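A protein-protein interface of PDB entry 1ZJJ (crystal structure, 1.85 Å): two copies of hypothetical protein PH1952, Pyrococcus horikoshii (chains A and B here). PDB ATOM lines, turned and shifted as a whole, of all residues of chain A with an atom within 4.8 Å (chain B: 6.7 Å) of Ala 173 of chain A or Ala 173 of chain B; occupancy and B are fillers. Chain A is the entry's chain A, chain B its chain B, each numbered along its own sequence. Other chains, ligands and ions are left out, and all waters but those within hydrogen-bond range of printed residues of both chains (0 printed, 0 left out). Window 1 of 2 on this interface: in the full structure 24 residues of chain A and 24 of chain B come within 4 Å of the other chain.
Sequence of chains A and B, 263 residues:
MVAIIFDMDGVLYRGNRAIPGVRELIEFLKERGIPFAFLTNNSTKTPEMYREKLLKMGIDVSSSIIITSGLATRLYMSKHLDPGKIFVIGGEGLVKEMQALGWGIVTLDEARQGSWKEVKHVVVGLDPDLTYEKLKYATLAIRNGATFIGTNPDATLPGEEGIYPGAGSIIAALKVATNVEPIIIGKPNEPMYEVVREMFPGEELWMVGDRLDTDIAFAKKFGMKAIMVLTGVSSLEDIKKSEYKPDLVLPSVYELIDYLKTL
CB of Ala 173 of chain B touches O of Ser 169 of chain A, at 3.2 Å. Ser 169 of chain A touches Val 176 of chain B. Ala 172 of chain A touches Val 176 of chain B (CB to CG2, 3.7 Å). CB of Ala 173 of chain A touches CB of Ala 173 of chain B, 3.96 Å away. Val 176 of chain A touches Ala 155 of chain B. CG1 of Val 176 of chain A touches CA of Ser 169 of chain B, 3.9 Å away. Val 176 of chain A touches Ala 172 of chain B (CG2 to CB, 3.6 Å). Ala 177 of chain A touches Ala 155 of chain B.
Ala 173 of chain A touches just these residues of chain B: Ser 169 and Ala 173. Ala 173 of chain B touches just these residues of chain A: Ser 169 and Ala 173. Of the printed residues of chain B, Ala 177 of chain A touches Ala 155. Printed residues of chain A within 4 Å of Ser 169 of chain B: Ala 173 (3.0 Å) and Val 176 (3.9 Å). Of the printed residues of chain A, Ala 155 of chain B touches Val 176 and Ala 177. Of the printed residues of chain B, Ser 169 of chain A touches Ala 173 and Val 176. Gly 168 of chain B touches none of the printed residues of chain A. The nearest residue of chain B that does not touch Ala 173 of chain A is Ala 172 of chain B (4.6 Å). The nearest printed residue of chain A that does not touch Ala 173 of chain B is Ala 172 of chain A (4.8 Å). The nearest printed residue of chain B that does not touch Ala 172 of chain A is Ala 172 of chain B (4.4 Å).
Printed residues of chain A that touch a printed residue of chain B: Ser 169, Ala 172, Ala 173, Val 176 and Ala 177. Of the 17 printed residues of chain B, 5 touch a printed residue of chain A. Among the printed residues, 9 pairs touch across the chains. Among the printed residues, no Asp or Glu carboxylate lies within 4 Å of a Lys or Arg side-chain nitrogen of the other chain.
Ser 169 of chain A touches Ala 173 of chain B, and with the chains exchanged Ala 173 of chain A touches Ser 169 of chain B. Ser 169 of chain A touches Val 176 of chain B, and with the chains exchanged Val 176 of chain A touches Ser 169 of chain B. Ala 172 of chain A touches Val 176 of chain B, and with the chains exchanged Val 176 of chain A touches Ala 172 of chain B. Ala 173 of chain A touches its own counterpart, Ala 173 of chain B. 9 positions are printed for both chains. Of the 9 pairs that touch across the chains among the printed residues, 7 have their exchanged pair printed and touching as well.
O of Ala 173 of chain A sits at hydrogen-bond distance from OG of Ser 169 of chain B, at 3.0 Å.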
ATOM      1  N   SER A 169      11.565  28.808  12.438  1.00  0.00           N
ATOM      2  CA  SER A 169      11.554  28.671  13.887  1.00  0.00           C
ATOM      3  C   SER A 169      12.932  28.234  14.389  1.00  0.00           C
ATOM      4  O   SER A 169      13.374  28.658  15.458  1.00  0.00           O
ATOM      5  CB  SER A 169      10.451  27.689  14.330  1.00  0.00           C
ATOM      6  OG  SER A 169      10.940  26.378  14.541  1.00  0.00           O
ATOM      7  N   ILE A 170      13.616  27.402  13.609  1.00  0.00           N
ATOM      8  CA  ILE A 170      14.949  26.950  13.990  1.00  0.00           C
ATOM      9  C   ILE A 170      15.902  28.140  13.833  1.00  0.00           C
ATOM     10  O   ILE A 170      16.735  28.405  14.706  1.00  0.00           O
ATOM     11  CB  ILE A 170      15.418  25.762  13.106  1.00  0.00           C
ATOM     12  CG1 ILE A 170      14.452  24.579  13.276  1.00  0.00           C
ATOM     13  CG2 ILE A 170      16.821  25.325  13.510  1.00  0.00           C
ATOM     14  CD1 ILE A 170      14.855  23.339  12.511  1.00  0.00           C
ATOM     15  N   ILE A 171      15.754  28.867  12.731  1.00  0.00           N
ATOM     16  CA  ILE A 171      16.583  30.043  12.469  1.00  0.00           C
ATOM     17  C   ILE A 171      16.389  31.077  13.585  1.00  0.00           C
ATOM     18  O   ILE A 171      17.337  31.749  13.999  1.00  0.00           O
ATOM     19  CB  ILE A 171      16.223  30.672  11.094  1.00  0.00           C
ATOM     20  CG1 ILE A 171      16.674  29.723   9.975  1.00  0.00           C
ATOM     21  CG2 ILE A 171      16.869  32.053  10.941  1.00  0.00           C
ATOM     22  CD1 ILE A 171      16.024  29.979   8.641  1.00  0.00           C
ATOM     23  N   ALA A 172      15.164  31.185  14.085  1.00  0.00           N
ATOM     24  CA  ALA A 172      14.854  32.139  15.150  1.00  0.00           C
ATOM     25  C   ALA A 172      15.606  31.809  16.441  1.00  0.00           C
ATOM     26  O   ALA A 172      16.110  32.708  17.123  1.00  0.00           O
ATOM     27  CB  ALA A 172      13.355  32.160  15.408  1.00  0.00           C
ATOM     28  N   ALA A 173      15.672  30.523  16.777  1.00  0.00           N
ATOM     29  CA  ALA A 173      16.377  30.095  17.980  1.00  0.00           C
ATOM     30  C   ALA A 173      17.853  30.504  17.903  1.00  0.00           C
ATOM     31  O   ALA A 173      18.434  30.976  18.884  1.00  0.00           O
ATOM     32  CB  ALA A 173      16.263  28.585  18.144  1.00  0.00           C
ATOM     33  N   LEU A 174      18.450  30.322  16.731  1.00  0.00           N
ATOM     34  CA  LEU A 174      19.861  30.655  16.535  1.00  0.00           C
ATOM     35  C   LEU A 174      20.102  32.155  16.512  1.00  0.00           C
ATOM     36  O   LEU A 174      21.165  32.621  16.922  1.00  0.00           O
ATOM     37  CB  LEU A 174      20.377  30.012  15.250  1.00  0.00           C
ATOM     38  CG  LEU A 174      20.457  28.482  15.300  1.00  0.00           C
ATOM     39  CD1 LEU A 174      20.726  27.925  13.914  1.00  0.00           C
ATOM     40  CD2 LEU A 174      21.552  28.053  16.277  1.00  0.00           C
ATOM     41  N   LYS A 175      19.126  32.915  16.023  1.00  0.00           N
ATOM     42  CA  LYS A 175      19.253  34.367  15.998  1.00  0.00           C
ATOM     43  C   LYS A 175      19.336  34.843  17.447  1.00  0.00           C
ATOM     44  O   LYS A 175      20.142  35.715  17.787  1.00  0.00           O
ATOM     45  CB  LYS A 175      18.035  34.986  15.303  1.00  0.00           C
ATOM     46  CG  LYS A 175      18.016  36.512  15.261  1.00  0.00           C
ATOM     47  CD  LYS A 175      16.770  37.016  14.526  1.00  0.00           C
ATOM     48  CE  LYS A 175      15.491  36.474  15.164  1.00  0.00           C
ATOM     49  NZ  LYS A 175      14.259  36.798  14.383  1.00  0.00           N
ATOM     50  N   VAL A 176      18.502  34.261  18.304  1.00  0.00           N
ATOM     51  CA  VAL A 176      18.482  34.621  19.719  1.00  0.00           C
ATOM     52  C   VAL A 176      19.765  34.207  20.427  1.00  0.00           C
ATOM     53  O   VAL A 176      20.304  34.958  21.237  1.00  0.00           O
ATOM     54  CB  VAL A 176      17.279  33.971  20.445  1.00  0.00           C
ATOM     55  CG1 VAL A 176      17.442  34.093  21.965  1.00  0.00           C
ATOM     56  CG2 VAL A 176      15.993  34.646  20.005  1.00  0.00           C
ATOM     57  N   ALA A 177      20.261  33.018  20.106  1.00  0.00           N
ATOM     58  CA  ALA A 177      21.471  32.497  20.731  1.00  0.00           C
ATOM     59  C   ALA A 177      22.765  33.166  20.271  1.00  0.00           C
ATOM     60  O   ALA A 177      23.750  33.182  21.007  1.00  0.00           O
ATOM     61  CB  ALA A 177      21.570  30.996  20.491  1.00  0.00           C
ATOM     62  N   LEU B 130      17.386  18.584  23.615  1.00  0.00           N
ATOM     63  CA  LEU B 130      16.287  19.013  22.755  1.00  0.00           C
ATOM     64  C   LEU B 130      16.331  18.296  21.408  1.00  0.00           C
ATOM     65  O   LEU B 130      17.402  18.002  20.877  1.00  0.00           O
ATOM     66  CB  LEU B 130      16.349  20.531  22.509  1.00  0.00           C
ATOM     67  CG  LEU B 130      15.212  21.113  21.656  1.00  0.00           C
ATOM     68  CD1 LEU B 130      13.910  21.020  22.442  1.00  0.00           C
ATOM     69  CD2 LEU B 130      15.499  22.567  21.282  1.00  0.00           C
ATOM     70  N   LEU B 135       9.978  19.779  19.879  1.00  0.00           N
ATOM     71  CA  LEU B 135       9.428  21.046  19.401  1.00  0.00           C
ATOM     72  C   LEU B 135       8.106  20.818  18.670  1.00  0.00           C
ATOM     73  O   LEU B 135       7.180  21.628  18.761  1.00  0.00           O
ATOM     74  CB  LEU B 135      10.407  21.733  18.441  1.00  0.00           C
ATOM     75  CG  LEU B 135      11.714  22.231  19.051  1.00  0.00           C
ATOM     76  CD1 LEU B 135      12.599  22.808  17.954  1.00  0.00           C
ATOM     77  CD2 LEU B 135      11.408  23.286  20.114  1.00  0.00           C
ATOM     78  N   THR B 139       4.577  22.331  19.866  1.00  0.00           N
ATOM     79  CA  THR B 139       3.900  23.231  18.947  1.00  0.00           C
ATOM     80  C   THR B 139       2.462  22.771  18.705  1.00  0.00           C
ATOM     81  O   THR B 139       1.526  23.574  18.744  1.00  0.00           O
ATOM     82  CB  THR B 139       4.658  23.302  17.596  1.00  0.00           C
ATOM     83  OG1 THR B 139       5.918  23.951  17.798  1.00  0.00           O
ATOM     84  CG2 THR B 139       3.861  24.067  16.558  1.00  0.00           C
ATOM     85  N   PHE B 148       1.394  28.084  27.027  1.00  0.00           N
ATOM     86  CA  PHE B 148       2.784  28.136  26.587  1.00  0.00           C
ATOM     87  C   PHE B 148       3.526  28.852  27.717  1.00  0.00           C
ATOM     88  O   PHE B 148       3.392  30.064  27.886  1.00  0.00           O
ATOM     89  CB  PHE B 148       2.863  28.923  25.268  1.00  0.00           C
ATOM     90  CG  PHE B 148       4.257  29.080  24.698  1.00  0.00           C
ATOM     91  CD1 PHE B 148       5.354  28.419  25.245  1.00  0.00           C
ATOM     92  CD2 PHE B 148       4.457  29.897  23.585  1.00  0.00           C
ATOM     93  CE1 PHE B 148       6.637  28.574  24.687  1.00  0.00           C
ATOM     94  CE2 PHE B 148       5.730  30.059  23.020  1.00  0.00           C
ATOM     95  CZ  PHE B 148       6.819  29.400  23.568  1.00  0.00           C
ATOM     96  N   ALA B 155      18.764  34.221  26.643  1.00  0.00           N
ATOM     97  CA  ALA B 155      19.105  33.833  25.287  1.00  0.00           C
ATOM     98  C   ALA B 155      20.239  32.815  25.297  1.00  0.00           C
ATOM     99  O   ALA B 155      20.301  31.948  24.427  1.00  0.00           O
ATOM    100  CB  ALA B 155      19.537  35.060  24.494  1.00  0.00           C
ATOM    101  N   PRO B 165      23.294  27.932  23.713  1.00  0.00           N
ATOM    102  CA  PRO B 165      21.907  28.391  23.588  1.00  0.00           C
ATOM    103  C   PRO B 165      21.188  28.226  24.915  1.00  0.00           C
ATOM    104  O   PRO B 165      21.327  27.194  25.577  1.00  0.00           O
ATOM    105  CB  PRO B 165      21.324  27.461  22.523  1.00  0.00           C
ATOM    106  CG  PRO B 165      22.486  27.107  21.694  1.00  0.00           C
ATOM    107  CD  PRO B 165      23.589  26.896  22.704  1.00  0.00           C
ATOM    108  N   GLY B 168      15.722  30.790  26.473  1.00  0.00           N
ATOM    109  CA  GLY B 168      15.104  31.795  25.624  1.00  0.00           C
ATOM    110  C   GLY B 168      15.208  31.454  24.150  1.00  0.00           C
ATOM    111  O   GLY B 168      14.346  31.819  23.347  1.00  0.00           O
ATOM    112  N   SER B 169      16.277  30.747  23.806  1.00  0.00           N
ATOM    113  CA  SER B 169      16.551  30.320  22.440  1.00  0.00           C
ATOM    114  C   SER B 169      15.500  29.302  22.019  1.00  0.00           C
ATOM    115  O   SER B 169      14.966  29.360  20.912  1.00  0.00           O
ATOM    116  CB  SER B 169      17.947  29.676  22.372  1.00  0.00           C
ATOM    117  OG  SER B 169      18.146  28.982  21.155  1.00  0.00           O
ATOM    118  N   ILE B 170      15.218  28.366  22.917  1.00  0.00           N
ATOM    119  CA  ILE B 170      14.238  27.321  22.647  1.00  0.00           C
ATOM    120  C   ILE B 170      12.836  27.915  22.637  1.00  0.00           C
ATOM    121  O   ILE B 170      12.020  27.614  21.760  1.00  0.00           O
ATOM    122  CB  ILE B 170      14.336  26.206  23.708  1.00  0.00           C
ATOM    123  CG1 ILE B 170      15.762  25.656  23.718  1.00  0.00           C
ATOM    124  CG2 ILE B 170      13.330  25.092  23.408  1.00  0.00           C
ATOM    125  CD1 ILE B 170      16.038  24.607  24.778  1.00  0.00           C
ATOM    126  N   ILE B 171      12.565  28.777  23.613  1.00  0.00           N
ATOM    127  CA  ILE B 171      11.268  29.429  23.719  1.00  0.00           C
ATOM    128  C   ILE B 171      10.994  30.253  22.469  1.00  0.00           C
ATOM    129  O   ILE B 171       9.866  30.295  21.981  1.00  0.00           O
ATOM    130  CB  ILE B 171      11.206  30.343  24.974  1.00  0.00           C
ATOM    131  CG1 ILE B 171      11.172  29.477  26.236  1.00  0.00           C
ATOM    132  CG2 ILE B 171       9.984  31.253  24.914  1.00  0.00           C
ATOM    133  CD1 ILE B 171      11.475  30.233  27.510  1.00  0.00           C
ATOM    134  N   ALA B 172      12.031  30.892  21.935  1.00  0.00           N
ATOM    135  CA  ALA B 172      11.876  31.714  20.741  1.00  0.00           C
ATOM    136  C   ALA B 172      11.403  30.880  19.559  1.00  0.00           C
ATOM    137  O   ALA B 172      10.522  31.304  18.810  1.00  0.00           O
ATOM    138  CB  ALA B 172      13.195  32.407  20.403  1.00  0.00           C
ATOM    139  N   ALA B 173      11.991  29.700  19.389  1.00  0.00           N
ATOM    140  CA  ALA B 173      11.604  28.811  18.297  1.00  0.00           C
ATOM    141  C   ALA B 173      10.120  28.455  18.394  1.00  0.00           C
ATOM    142  O   ALA B 173       9.406  28.471  17.394  1.00  0.00           O
ATOM    143  CB  ALA B 173      12.445  27.543  18.329  1.00  0.00           C
ATOM    144  N   LEU B 174       9.655  28.144  19.602  1.00  0.00           N
ATOM    145  CA  LEU B 174       8.256  27.781  19.801  1.00  0.00           C
ATOM    146  C   LEU B 174       7.323  28.972  19.610  1.00  0.00           C
ATOM    147  O   LEU B 174       6.186  28.811  19.166  1.00  0.00           O
ATOM    148  CB  LEU B 174       8.070  27.160  21.183  1.00  0.00           C
ATOM    149  CG  LEU B 174       8.658  25.754  21.292  1.00  0.00           C
ATOM    150  CD1 LEU B 174       8.534  25.259  22.718  1.00  0.00           C
ATOM    151  CD2 LEU B 174       7.935  24.815  20.315  1.00  0.00           C
ATOM    152  N   LYS B 175       7.806  30.170  19.930  1.00  0.00           N
ATOM    153  CA  LYS B 175       7.006  31.379  19.744  1.00  0.00           C
ATOM    154  C   LYS B 175       6.735  31.548  18.246  1.00  0.00           C
ATOM    155  O   LYS B 175       5.623  31.890  17.835  1.00  0.00           O
ATOM    156  CB  LYS B 175       7.758  32.603  20.275  1.00  0.00           C
ATOM    157  CG  LYS B 175       7.004  33.920  20.122  1.00  0.00           C
ATOM    158  CD  LYS B 175       7.711  35.052  20.867  1.00  0.00           C
ATOM    159  CE  LYS B 175       9.101  35.312  20.295  1.00  0.00           C
ATOM    160  NZ  LYS B 175       9.915  36.266  21.104  1.00  0.00           N
ATOM    161  N   VAL B 176       7.761  31.306  17.436  1.00  0.00           N
ATOM    162  CA  VAL B 176       7.636  31.416  15.985  1.00  0.00           C
ATOM    163  C   VAL B 176       6.767  30.305  15.400  1.00  0.00           C
ATOM    164  O   VAL B 176       5.944  30.553  14.521  1.00  0.00           O
ATOM    165  CB  VAL B 176       9.023  31.386  15.307  1.00  0.00           C
ATOM    166  CG1 VAL B 176       8.881  31.179  13.800  1.00  0.00           C
ATOM    167  CG2 VAL B 176       9.738  32.689  15.583  1.00  0.00           C
ATOM    168  N   ALA B 177       6.940  29.087  15.902  1.00  0.00           N
ATOM    169  CA  ALA B 177       6.172  27.950  15.405  1.00  0.00           C
ATOM    170  C   ALA B 177       4.707  27.967  15.834  1.00  0.00           C
ATOM    171  O   ALA B 177       3.853  27.436  15.132  1.00  0.00           O
ATOM    172  CB  ALA B 177       6.827  26.654  15.851  1.00  0.00           C
ATOM    173  N   THR B 178       4.413  28.580  16.976  1.00  0.00           N
ATOM    174  CA  THR B 178       3.037  28.616  17.480  1.00  0.00           C
ATOM    175  C   THR B 178       2.332  29.940  17.260  1.00  0.00           C
ATOM    176  O   THR B 178       1.102  30.002  17.237  1.00  0.00           O
ATOM    177  CB  THR B 178       2.983  28.339  18.991  1.00  0.00           C
ATOM    178  OG1 THR B 178       3.588  29.434  19.698  1.00  0.00           O
ATOM    179  CG2 THR B 178       3.710  27.053  19.328  1.00  0.00           C
